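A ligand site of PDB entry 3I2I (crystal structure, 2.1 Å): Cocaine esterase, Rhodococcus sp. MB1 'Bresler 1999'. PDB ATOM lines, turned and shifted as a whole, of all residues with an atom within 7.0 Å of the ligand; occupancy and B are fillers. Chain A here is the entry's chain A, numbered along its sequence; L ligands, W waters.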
ATOM      1  N   PRO A  43      -1.319   5.434 -20.373  1.00  0.00           N
ATOM      2  CA  PRO A  43      -1.847   6.624 -21.059  1.00  0.00           C
ATOM      3  C   PRO A  43      -2.922   7.397 -20.272  1.00  0.00           C
ATOM      4  O   PRO A  43      -3.507   8.329 -20.797  1.00  0.00           O
ATOM      5  CB  PRO A  43      -2.477   6.040 -22.322  1.00  0.00           C
ATOM      6  CG  PRO A  43      -3.035   4.720 -21.860  1.00  0.00           C
ATOM      7  CD  PRO A  43      -2.099   4.222 -20.757  1.00  0.00           C
ATOM      8  N   TYR A  44      -3.185   6.987 -19.032  1.00  0.00           N
ATOM      9  CA  TYR A  44      -4.307   7.536 -18.269  1.00  0.00           C
ATOM     10  C   TYR A  44      -3.835   8.274 -17.014  1.00  0.00           C
ATOM     11  O   TYR A  44      -4.557   8.322 -16.011  1.00  0.00           O
ATOM     12  CB  TYR A  44      -5.269   6.406 -17.856  1.00  0.00           C
ATOM     13  CG  TYR A  44      -5.677   5.476 -18.994  1.00  0.00           C
ATOM     14  CD1 TYR A  44      -6.399   5.961 -20.095  1.00  0.00           C
ATOM     15  CD2 TYR A  44      -5.360   4.108 -18.950  1.00  0.00           C
ATOM     16  CE1 TYR A  44      -6.776   5.116 -21.133  1.00  0.00           C
ATOM     17  CE2 TYR A  44      -5.730   3.256 -19.984  1.00  0.00           C
ATOM     18  CZ  TYR A  44      -6.437   3.765 -21.071  1.00  0.00           C
ATOM     19  OH  TYR A  44      -6.822   2.936 -22.092  1.00  0.00           O
ATOM     20  N   GLN A  55      -7.949  -2.974 -10.874  1.00  0.00           N
ATOM     21  CA  GLN A  55      -8.116  -3.989 -11.913  1.00  0.00           C
ATOM     22  C   GLN A  55      -6.870  -4.875 -12.048  1.00  0.00           C
ATOM     23  O   GLN A  55      -6.842  -5.770 -12.891  1.00  0.00           O
ATOM     24  CB  GLN A  55      -8.439  -3.311 -13.255  1.00  0.00           C
ATOM     25  CG  GLN A  55      -9.745  -2.502 -13.265  1.00  0.00           C
ATOM     26  CD  GLN A  55      -9.562  -1.094 -13.795  1.00  0.00           C
ATOM     27  OE1 GLN A  55      -9.058  -0.886 -14.900  1.00  0.00           O
ATOM     28  NE2 GLN A  55      -9.963  -0.106 -12.987  1.00  0.00           N
ATOM     29  N   HIS A  87      -0.428   3.494 -29.876  1.00  0.00           N
ATOM     30  CA  HIS A  87       0.361   2.318 -30.292  1.00  0.00           C
ATOM     31  C   HIS A  87       1.697   2.574 -31.027  1.00  0.00           C
ATOM     32  O   HIS A  87       2.648   1.796 -30.862  1.00  0.00           O
ATOM     33  CB  HIS A  87      -0.469   1.329 -31.151  1.00  0.00           C
ATOM     34  CG  HIS A  87      -1.867   1.063 -30.658  1.00  0.00           C
ATOM     35  ND1 HIS A  87      -2.148   0.720 -29.347  1.00  0.00           N
ATOM     36  CD2 HIS A  87      -3.055   1.055 -31.310  1.00  0.00           C
ATOM     37  CE1 HIS A  87      -3.457   0.527 -29.219  1.00  0.00           C
ATOM     38  NE2 HIS A  87      -4.027   0.710 -30.403  1.00  0.00           N
ATOM     39  N   VAL A 116      -2.798  -3.632 -16.878  1.00  0.00           N
ATOM     40  CA  VAL A 116      -4.003  -4.088 -17.513  1.00  0.00           C
ATOM     41  C   VAL A 116      -4.320  -3.225 -18.746  1.00  0.00           C
ATOM     42  O   VAL A 116      -4.011  -2.015 -18.784  1.00  0.00           O
ATOM     43  CB  VAL A 116      -5.188  -4.065 -16.458  1.00  0.00           C
ATOM     44  CG1 VAL A 116      -5.476  -2.651 -15.995  1.00  0.00           C
ATOM     45  CG2 VAL A 116      -6.432  -4.728 -16.984  1.00  0.00           C
ATOM     46  N   SER A 117      -4.918  -3.855 -19.761  1.00  0.00           N
ATOM     47  CA  SER A 117      -5.470  -3.155 -20.917  1.00  0.00           C
ATOM     48  C   SER A 117      -4.345  -2.543 -21.752  1.00  0.00           C
ATOM     49  O   SER A 117      -3.459  -3.267 -22.209  1.00  0.00           O
ATOM     50  CB  SER A 117      -6.540  -2.133 -20.466  1.00  0.00           C
ATOM     51  OG  SER A 117      -7.476  -1.868 -21.496  1.00  0.00           O
ATOM     52  N   TYR A 118      -4.341  -1.224 -21.919  1.00  0.00           N
ATOM     53  CA  TYR A 118      -3.258  -0.533 -22.640  1.00  0.00           C
ATOM     54  C   TYR A 118      -1.931  -0.716 -21.873  1.00  0.00           C
ATOM     55  O   TYR A 118      -0.860  -0.814 -22.464  1.00  0.00           O
ATOM     56  CB  TYR A 118      -3.604   0.941 -22.797  1.00  0.00           C
ATOM     57  CG  TYR A 118      -2.883   1.696 -23.882  1.00  0.00           C
ATOM     58  CD1 TYR A 118      -1.548   2.120 -23.713  1.00  0.00           C
ATOM     59  CD2 TYR A 118      -3.545   2.041 -25.071  1.00  0.00           C
ATOM     60  CE1 TYR A 118      -0.894   2.843 -24.701  1.00  0.00           C
ATOM     61  CE2 TYR A 118      -2.902   2.787 -26.056  1.00  0.00           C
ATOM     62  CZ  TYR A 118      -1.587   3.184 -25.870  1.00  0.00           C
ATOM     63  OH  TYR A 118      -0.940   3.900 -26.860  1.00  0.00           O
ATOM     64  N   LEU A 119      -2.023  -0.770 -20.542  1.00  0.00           N
ATOM     65  CA  LEU A 119      -0.857  -1.085 -19.694  1.00  0.00           C
ATOM     66  C   LEU A 119      -0.374  -2.542 -19.896  1.00  0.00           C
ATOM     67  O   LEU A 119       0.718  -2.898 -19.466  1.00  0.00           O
ATOM     68  CB  LEU A 119      -1.150  -0.808 -18.217  1.00  0.00           C
ATOM     69  CG  LEU A 119      -1.419   0.642 -17.751  1.00  0.00           C
ATOM     70  CD1 LEU A 119      -2.590   1.291 -18.503  1.00  0.00           C
ATOM     71  CD2 LEU A 119      -1.670   0.702 -16.250  1.00  0.00           C
ATOM     72  N   GLY A 120      -1.214  -3.372 -20.528  1.00  0.00           N
ATOM     73  CA  GLY A 120      -0.854  -4.747 -20.912  1.00  0.00           C
ATOM     74  C   GLY A 120      -0.315  -4.831 -22.345  1.00  0.00           C
ATOM     75  O   GLY A 120       0.684  -5.499 -22.599  1.00  0.00           O
ATOM     76  N   VAL A 121      -0.974  -4.144 -23.272  1.00  0.00           N
ATOM     77  CA  VAL A 121      -0.536  -4.096 -24.665  1.00  0.00           C
ATOM     78  C   VAL A 121       0.927  -3.590 -24.748  1.00  0.00           C
ATOM     79  O   VAL A 121       1.756  -4.163 -25.466  1.00  0.00           O
ATOM     80  CB  VAL A 121      -1.450  -3.169 -25.488  1.00  0.00           C
ATOM     81  CG1 VAL A 121      -0.885  -2.967 -26.915  1.00  0.00           C
ATOM     82  CG2 VAL A 121      -2.911  -3.681 -25.502  1.00  0.00           C
ATOM     83  N   MET A 141      -5.621  -8.600 -19.584  1.00  0.00           N
ATOM     84  CA  MET A 141      -6.720  -8.174 -20.462  1.00  0.00           C
ATOM     85  C   MET A 141      -6.143  -7.359 -21.668  1.00  0.00           C
ATOM     86  O   MET A 141      -6.535  -6.221 -21.889  1.00  0.00           O
ATOM     87  CB  MET A 141      -7.840  -7.439 -19.635  1.00  0.00           C
ATOM     88  CG  MET A 141      -8.641  -8.367 -18.724  1.00  0.00           C
ATOM     89  SD  MET A 141      -9.666  -7.439 -17.577  1.00  0.00           S
ATOM     90  CE  MET A 141     -11.178  -8.411 -17.564  1.00  0.00           C
ATOM     91  N   LEU A 146      -3.457  -5.692 -32.539  1.00  0.00           N
ATOM     92  CA  LEU A 146      -4.460  -4.650 -32.312  1.00  0.00           C
ATOM     93  C   LEU A 146      -5.614  -4.703 -33.304  1.00  0.00           C
ATOM     94  O   LEU A 146      -6.692  -4.202 -33.018  1.00  0.00           O
ATOM     95  CB  LEU A 146      -3.810  -3.257 -32.332  1.00  0.00           C
ATOM     96  CG  LEU A 146      -2.944  -2.851 -31.134  1.00  0.00           C
ATOM     97  CD1 LEU A 146      -3.632  -3.063 -29.778  1.00  0.00           C
ATOM     98  CD2 LEU A 146      -1.621  -3.568 -31.182  1.00  0.00           C
ATOM     99  N   ALA A 149      -7.790  -7.615 -31.628  1.00  0.00           N
ATOM    100  CA  ALA A 149      -8.446  -6.984 -30.476  1.00  0.00           C
ATOM    101  C   ALA A 149      -7.622  -5.767 -30.107  1.00  0.00           C
ATOM    102  O   ALA A 149      -6.408  -5.858 -29.998  1.00  0.00           O
ATOM    103  CB  ALA A 149      -8.557  -7.966 -29.263  1.00  0.00           C
ATOM    104  N   PRO A 150      -8.269  -4.648 -29.809  1.00  0.00           N
ATOM    105  CA  PRO A 150      -9.703  -4.448 -29.675  1.00  0.00           C
ATOM    106  C   PRO A 150     -10.413  -3.790 -30.869  1.00  0.00           C
ATOM    107  O   PRO A 150     -11.621  -3.560 -30.787  1.00  0.00           O
ATOM    108  CB  PRO A 150      -9.758  -3.488 -28.492  1.00  0.00           C
ATOM    109  CG  PRO A 150      -8.573  -2.559 -28.765  1.00  0.00           C
ATOM    110  CD  PRO A 150      -7.521  -3.432 -29.440  1.00  0.00           C
ATOM    111  N   TRP A 151      -9.693  -3.441 -31.946  1.00  0.00           N
ATOM    112  CA  TRP A 151     -10.282  -2.515 -32.950  1.00  0.00           C
ATOM    113  C   TRP A 151     -11.160  -3.182 -34.022  1.00  0.00           C
ATOM    114  O   TRP A 151     -12.235  -2.644 -34.371  1.00  0.00           O
ATOM    115  CB  TRP A 151      -9.222  -1.565 -33.539  1.00  0.00           C
ATOM    116  CG  TRP A 151      -8.438  -0.827 -32.472  1.00  0.00           C
ATOM    117  CD1 TRP A 151      -7.080  -0.779 -32.343  1.00  0.00           C
ATOM    118  CD2 TRP A 151      -8.972  -0.111 -31.335  1.00  0.00           C
ATOM    119  NE1 TRP A 151      -6.738  -0.068 -31.236  1.00  0.00           N
ATOM    120  CE2 TRP A 151      -7.872   0.358 -30.593  1.00  0.00           C
ATOM    121  CE3 TRP A 151     -10.275   0.154 -30.872  1.00  0.00           C
ATOM    122  CZ2 TRP A 151      -8.007   1.091 -29.403  1.00  0.00           C
ATOM    123  CZ3 TRP A 151     -10.421   0.899 -29.698  1.00  0.00           C
ATOM    124  CH2 TRP A 151      -9.296   1.352 -28.977  1.00  0.00           C
ATOM    125  N   ALA A 162     -16.226  -0.073 -29.179  1.00  0.00           N
ATOM    126  CA  ALA A 162     -14.908  -0.010 -28.556  1.00  0.00           C
ATOM    127  C   ALA A 162     -14.157   1.229 -29.048  1.00  0.00           C
ATOM    128  O   ALA A 162     -13.598   1.981 -28.239  1.00  0.00           O
ATOM    129  CB  ALA A 162     -14.103  -1.269 -28.847  1.00  0.00           C
ATOM    130  N   LEU A 163     -14.168   1.449 -30.356  1.00  0.00           N
ATOM    131  CA  LEU A 163     -13.464   2.580 -30.962  1.00  0.00           C
ATOM    132  C   LEU A 163     -13.984   3.942 -30.502  1.00  0.00           C
ATOM    133  O   LEU A 163     -13.221   4.795 -30.024  1.00  0.00           O
ATOM    134  CB  LEU A 163     -13.512   2.488 -32.473  1.00  0.00           C
ATOM    135  CG  LEU A 163     -12.830   3.677 -33.183  1.00  0.00           C
ATOM    136  CD1 LEU A 163     -11.301   3.651 -32.974  1.00  0.00           C
ATOM    137  CD2 LEU A 163     -13.189   3.697 -34.641  1.00  0.00           C
ATOM    138  N   GLY A 165     -16.031   4.636 -27.982  1.00  0.00           N
ATOM    139  CA  GLY A 165     -16.034   4.747 -26.538  1.00  0.00           C
ATOM    140  C   GLY A 165     -14.662   5.138 -26.022  1.00  0.00           C
ATOM    141  O   GLY A 165     -14.522   6.057 -25.222  1.00  0.00           O
ATOM    142  N   TRP A 166     -13.649   4.428 -26.493  1.00  0.00           N
ATOM    143  CA  TRP A 166     -12.295   4.689 -26.045  1.00  0.00           C
ATOM    144  C   TRP A 166     -11.777   6.048 -26.528  1.00  0.00           C
ATOM    145  O   TRP A 166     -11.087   6.770 -25.792  1.00  0.00           O
ATOM    146  CB  TRP A 166     -11.368   3.579 -26.511  1.00  0.00           C
ATOM    147  CG  TRP A 166      -9.994   3.700 -25.884  1.00  0.00           C
ATOM    148  CD1 TRP A 166      -9.662   3.453 -24.572  1.00  0.00           C
ATOM    149  CD2 TRP A 166      -8.790   4.093 -26.538  1.00  0.00           C
ATOM    150  NE1 TRP A 166      -8.315   3.659 -24.381  1.00  0.00           N
ATOM    151  CE2 TRP A 166      -7.750   4.049 -25.570  1.00  0.00           C
ATOM    152  CE3 TRP A 166      -8.466   4.466 -27.847  1.00  0.00           C
ATOM    153  CZ2 TRP A 166      -6.419   4.369 -25.868  1.00  0.00           C
ATOM    154  CZ3 TRP A 166      -7.135   4.800 -28.147  1.00  0.00           C
ATOM    155  CH2 TRP A 166      -6.133   4.758 -27.162  1.00  0.00           C
ATOM    156  N   LEU A 169     -13.116   8.704 -24.371  1.00  0.00           N
ATOM    157  CA  LEU A 169     -12.364   8.668 -23.109  1.00  0.00           C
ATOM    158  C   LEU A 169     -10.992   9.341 -23.218  1.00  0.00           C
ATOM    159  O   LEU A 169     -10.618  10.172 -22.397  1.00  0.00           O
ATOM    160  CB  LEU A 169     -12.216   7.213 -22.633  1.00  0.00           C
ATOM    161  CG  LEU A 169     -12.278   6.996 -21.127  1.00  0.00           C
ATOM    162  CD1 LEU A 169     -13.711   7.310 -20.615  1.00  0.00           C
ATOM    163  CD2 LEU A 169     -11.868   5.555 -20.773  1.00  0.00           C
ATOM    164  N   PHE A 261     -10.794  -8.518 -24.974  1.00  0.00           N
ATOM    165  CA  PHE A 261      -9.467  -9.051 -25.360  1.00  0.00           C
ATOM    166  C   PHE A 261      -9.281 -10.562 -25.199  1.00  0.00           C
ATOM    167  O   PHE A 261      -8.185 -11.063 -25.434  1.00  0.00           O
ATOM    168  CB  PHE A 261      -8.384  -8.371 -24.532  1.00  0.00           C
ATOM    169  CG  PHE A 261      -8.144  -6.923 -24.870  1.00  0.00           C
ATOM    170  CD1 PHE A 261      -8.817  -5.911 -24.188  1.00  0.00           C
ATOM    171  CD2 PHE A 261      -7.234  -6.570 -25.868  1.00  0.00           C
ATOM    172  CE1 PHE A 261      -8.567  -4.546 -24.499  1.00  0.00           C
ATOM    173  CE2 PHE A 261      -6.977  -5.225 -26.175  1.00  0.00           C
ATOM    174  CZ  PHE A 261      -7.650  -4.213 -25.493  1.00  0.00           C
ATOM    175  N   HIS A 287     -14.479  -6.045 -19.294  1.00  0.00           N
ATOM    176  CA  HIS A 287     -13.384  -5.096 -19.139  1.00  0.00           C
ATOM    177  C   HIS A 287     -13.627  -4.089 -18.028  1.00  0.00           C
ATOM    178  O   HIS A 287     -12.701  -3.671 -17.340  1.00  0.00           O
ATOM    179  CB  HIS A 287     -13.145  -4.363 -20.463  1.00  0.00           C
ATOM    180  CG  HIS A 287     -11.731  -3.955 -20.695  1.00  0.00           C
ATOM    181  ND1 HIS A 287     -10.712  -4.857 -20.889  1.00  0.00           N
ATOM    182  CD2 HIS A 287     -11.163  -2.720 -20.772  1.00  0.00           C
ATOM    183  CE1 HIS A 287      -9.574  -4.204 -21.081  1.00  0.00           C
ATOM    184  NE2 HIS A 287      -9.825  -2.906 -21.013  1.00  0.00           N
ATOM    185  N   LEU A 407     -17.321  -3.470 -24.740  1.00  0.00           N
ATOM    186  CA  LEU A 407     -16.308  -2.709 -23.995  1.00  0.00           C
ATOM    187  C   LEU A 407     -16.843  -1.435 -23.333  1.00  0.00           C
ATOM    188  O   LEU A 407     -16.646  -1.227 -22.135  1.00  0.00           O
ATOM    189  CB  LEU A 407     -15.096  -2.376 -24.888  1.00  0.00           C
ATOM    190  CG  LEU A 407     -14.159  -3.580 -25.154  1.00  0.00           C
ATOM    191  CD1 LEU A 407     -13.130  -3.282 -26.194  1.00  0.00           C
ATOM    192  CD2 LEU A 407     -13.452  -3.995 -23.894  1.00  0.00           C
ATOM    193  N   PHE A 408     -17.515  -0.595 -24.121  1.00  0.00           N
ATOM    194  CA  PHE A 408     -18.003   0.716 -23.619  1.00  0.00           C
ATOM    195  C   PHE A 408     -19.509   0.870 -23.661  1.00  0.00           C
ATOM    196  O   PHE A 408     -20.083   1.504 -22.770  1.00  0.00           O
ATOM    197  CB  PHE A 408     -17.305   1.875 -24.329  1.00  0.00           C
ATOM    198  CG  PHE A 408     -15.839   1.934 -24.070  1.00  0.00           C
ATOM    199  CD1 PHE A 408     -15.352   2.486 -22.884  1.00  0.00           C
ATOM    200  CD2 PHE A 408     -14.935   1.408 -24.981  1.00  0.00           C
ATOM    201  CE1 PHE A 408     -13.976   2.515 -22.625  1.00  0.00           C
ATOM    202  CE2 PHE A 408     -13.569   1.417 -24.713  1.00  0.00           C
ATOM    203  CZ  PHE A 408     -13.091   1.981 -23.542  1.00  0.00           C
HETATM  204  O1  LIG L   1      -6.800   0.559 -21.245  1.00  0.00           O
HETATM  205  C1  LIG L   1      -7.548  -0.370 -22.088  1.00  0.00           C
HETATM  206  O2  LIG L   1      -8.980  -0.039 -22.470  1.00  0.00           O
HETATM  207  O3  LIG L   1      -6.836  -0.581 -23.401  1.00  0.00           O
HETATM  208  C2  LIG L   1      -7.791  -0.591 -24.458  1.00  0.00           C
HETATM  209  C3  LIG L   1      -7.161   0.158 -25.634  1.00  0.00           C
HETATM  210  S1  LIG L   1      -5.823  -0.819 -26.417  1.00  0.00           S
HETATM  211  C4  LIG L   1      -9.070   0.037 -23.900  1.00  0.00           C
HETATM  212  C5  LIG L   1     -10.344  -0.701 -24.287  1.00  0.00           C
HETATM  213  S2  LIG L   1     -10.730  -0.515 -26.061  1.00  0.00           S
HETATM  214  O   HOH W   1     -10.383   1.722 -21.096  1.00  0.00           O
HETATM  215  O   HOH W   2      -8.032   0.585 -18.750  1.00  0.00           O
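The side-chain hydroxyl of Tyr 118 is in hydrogen-bond range of the backbone NH of His 87 (3.1 Å).
NE1 of Trp 151 is in hydrogen-bond range of NE2 of His 87 (2.9 Å).
N of Trp 151 lies within hydrogen-bond range of O of Leu 146, at 3.3 Å.
NE2 of His 287 is in hydrogen-bond range of OG of Ser 117, 2.6 Å away.
The side-chain hydroxyl of Tyr 44 sits at hydrogen-bond distance from the indole nitrogen of Trp 166.
A carbon (C1) of the ligand is covalently linked to the side-chain hydroxyl (OG) of Ser 117, at 1.6 Å.
OH of Tyr 44 is in hydrogen-bond range of O1 of the ligand (2.5 Å).
An oxygen (O3) of the ligand sits at hydrogen-bond distance from the backbone NH (N) of Tyr 118, at 3.0 Å.
An oxygen (O2) of the ligand sits at hydrogen-bond distance from a ring nitrogen (NE2) of His 287.
Residues that only touch the ligand: Trp 166 (3.5 Å), Leu 407 (3.7 Å), Phe 408 (3.7 Å), Trp 151 (3.7 Å), Phe 261 (3.8 Å), His 87 (3.9 Å) and Pro 150 (3.96 Å).
Hydrophobic or aromatic side chains that line the ligand: Tyr 44, His 87, Tyr 118, Pro 150, Trp 151, Trp 166, Phe 261, His 287, Leu 407 and Phe 408.
11 residues have an atom within 4 Å of the ligand: Tyr 44, His 87, Ser 117, Tyr 118, Pro 150, Trp 151, Trp 166, Phe 261, His 287, Leu 407 and Phe 408.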
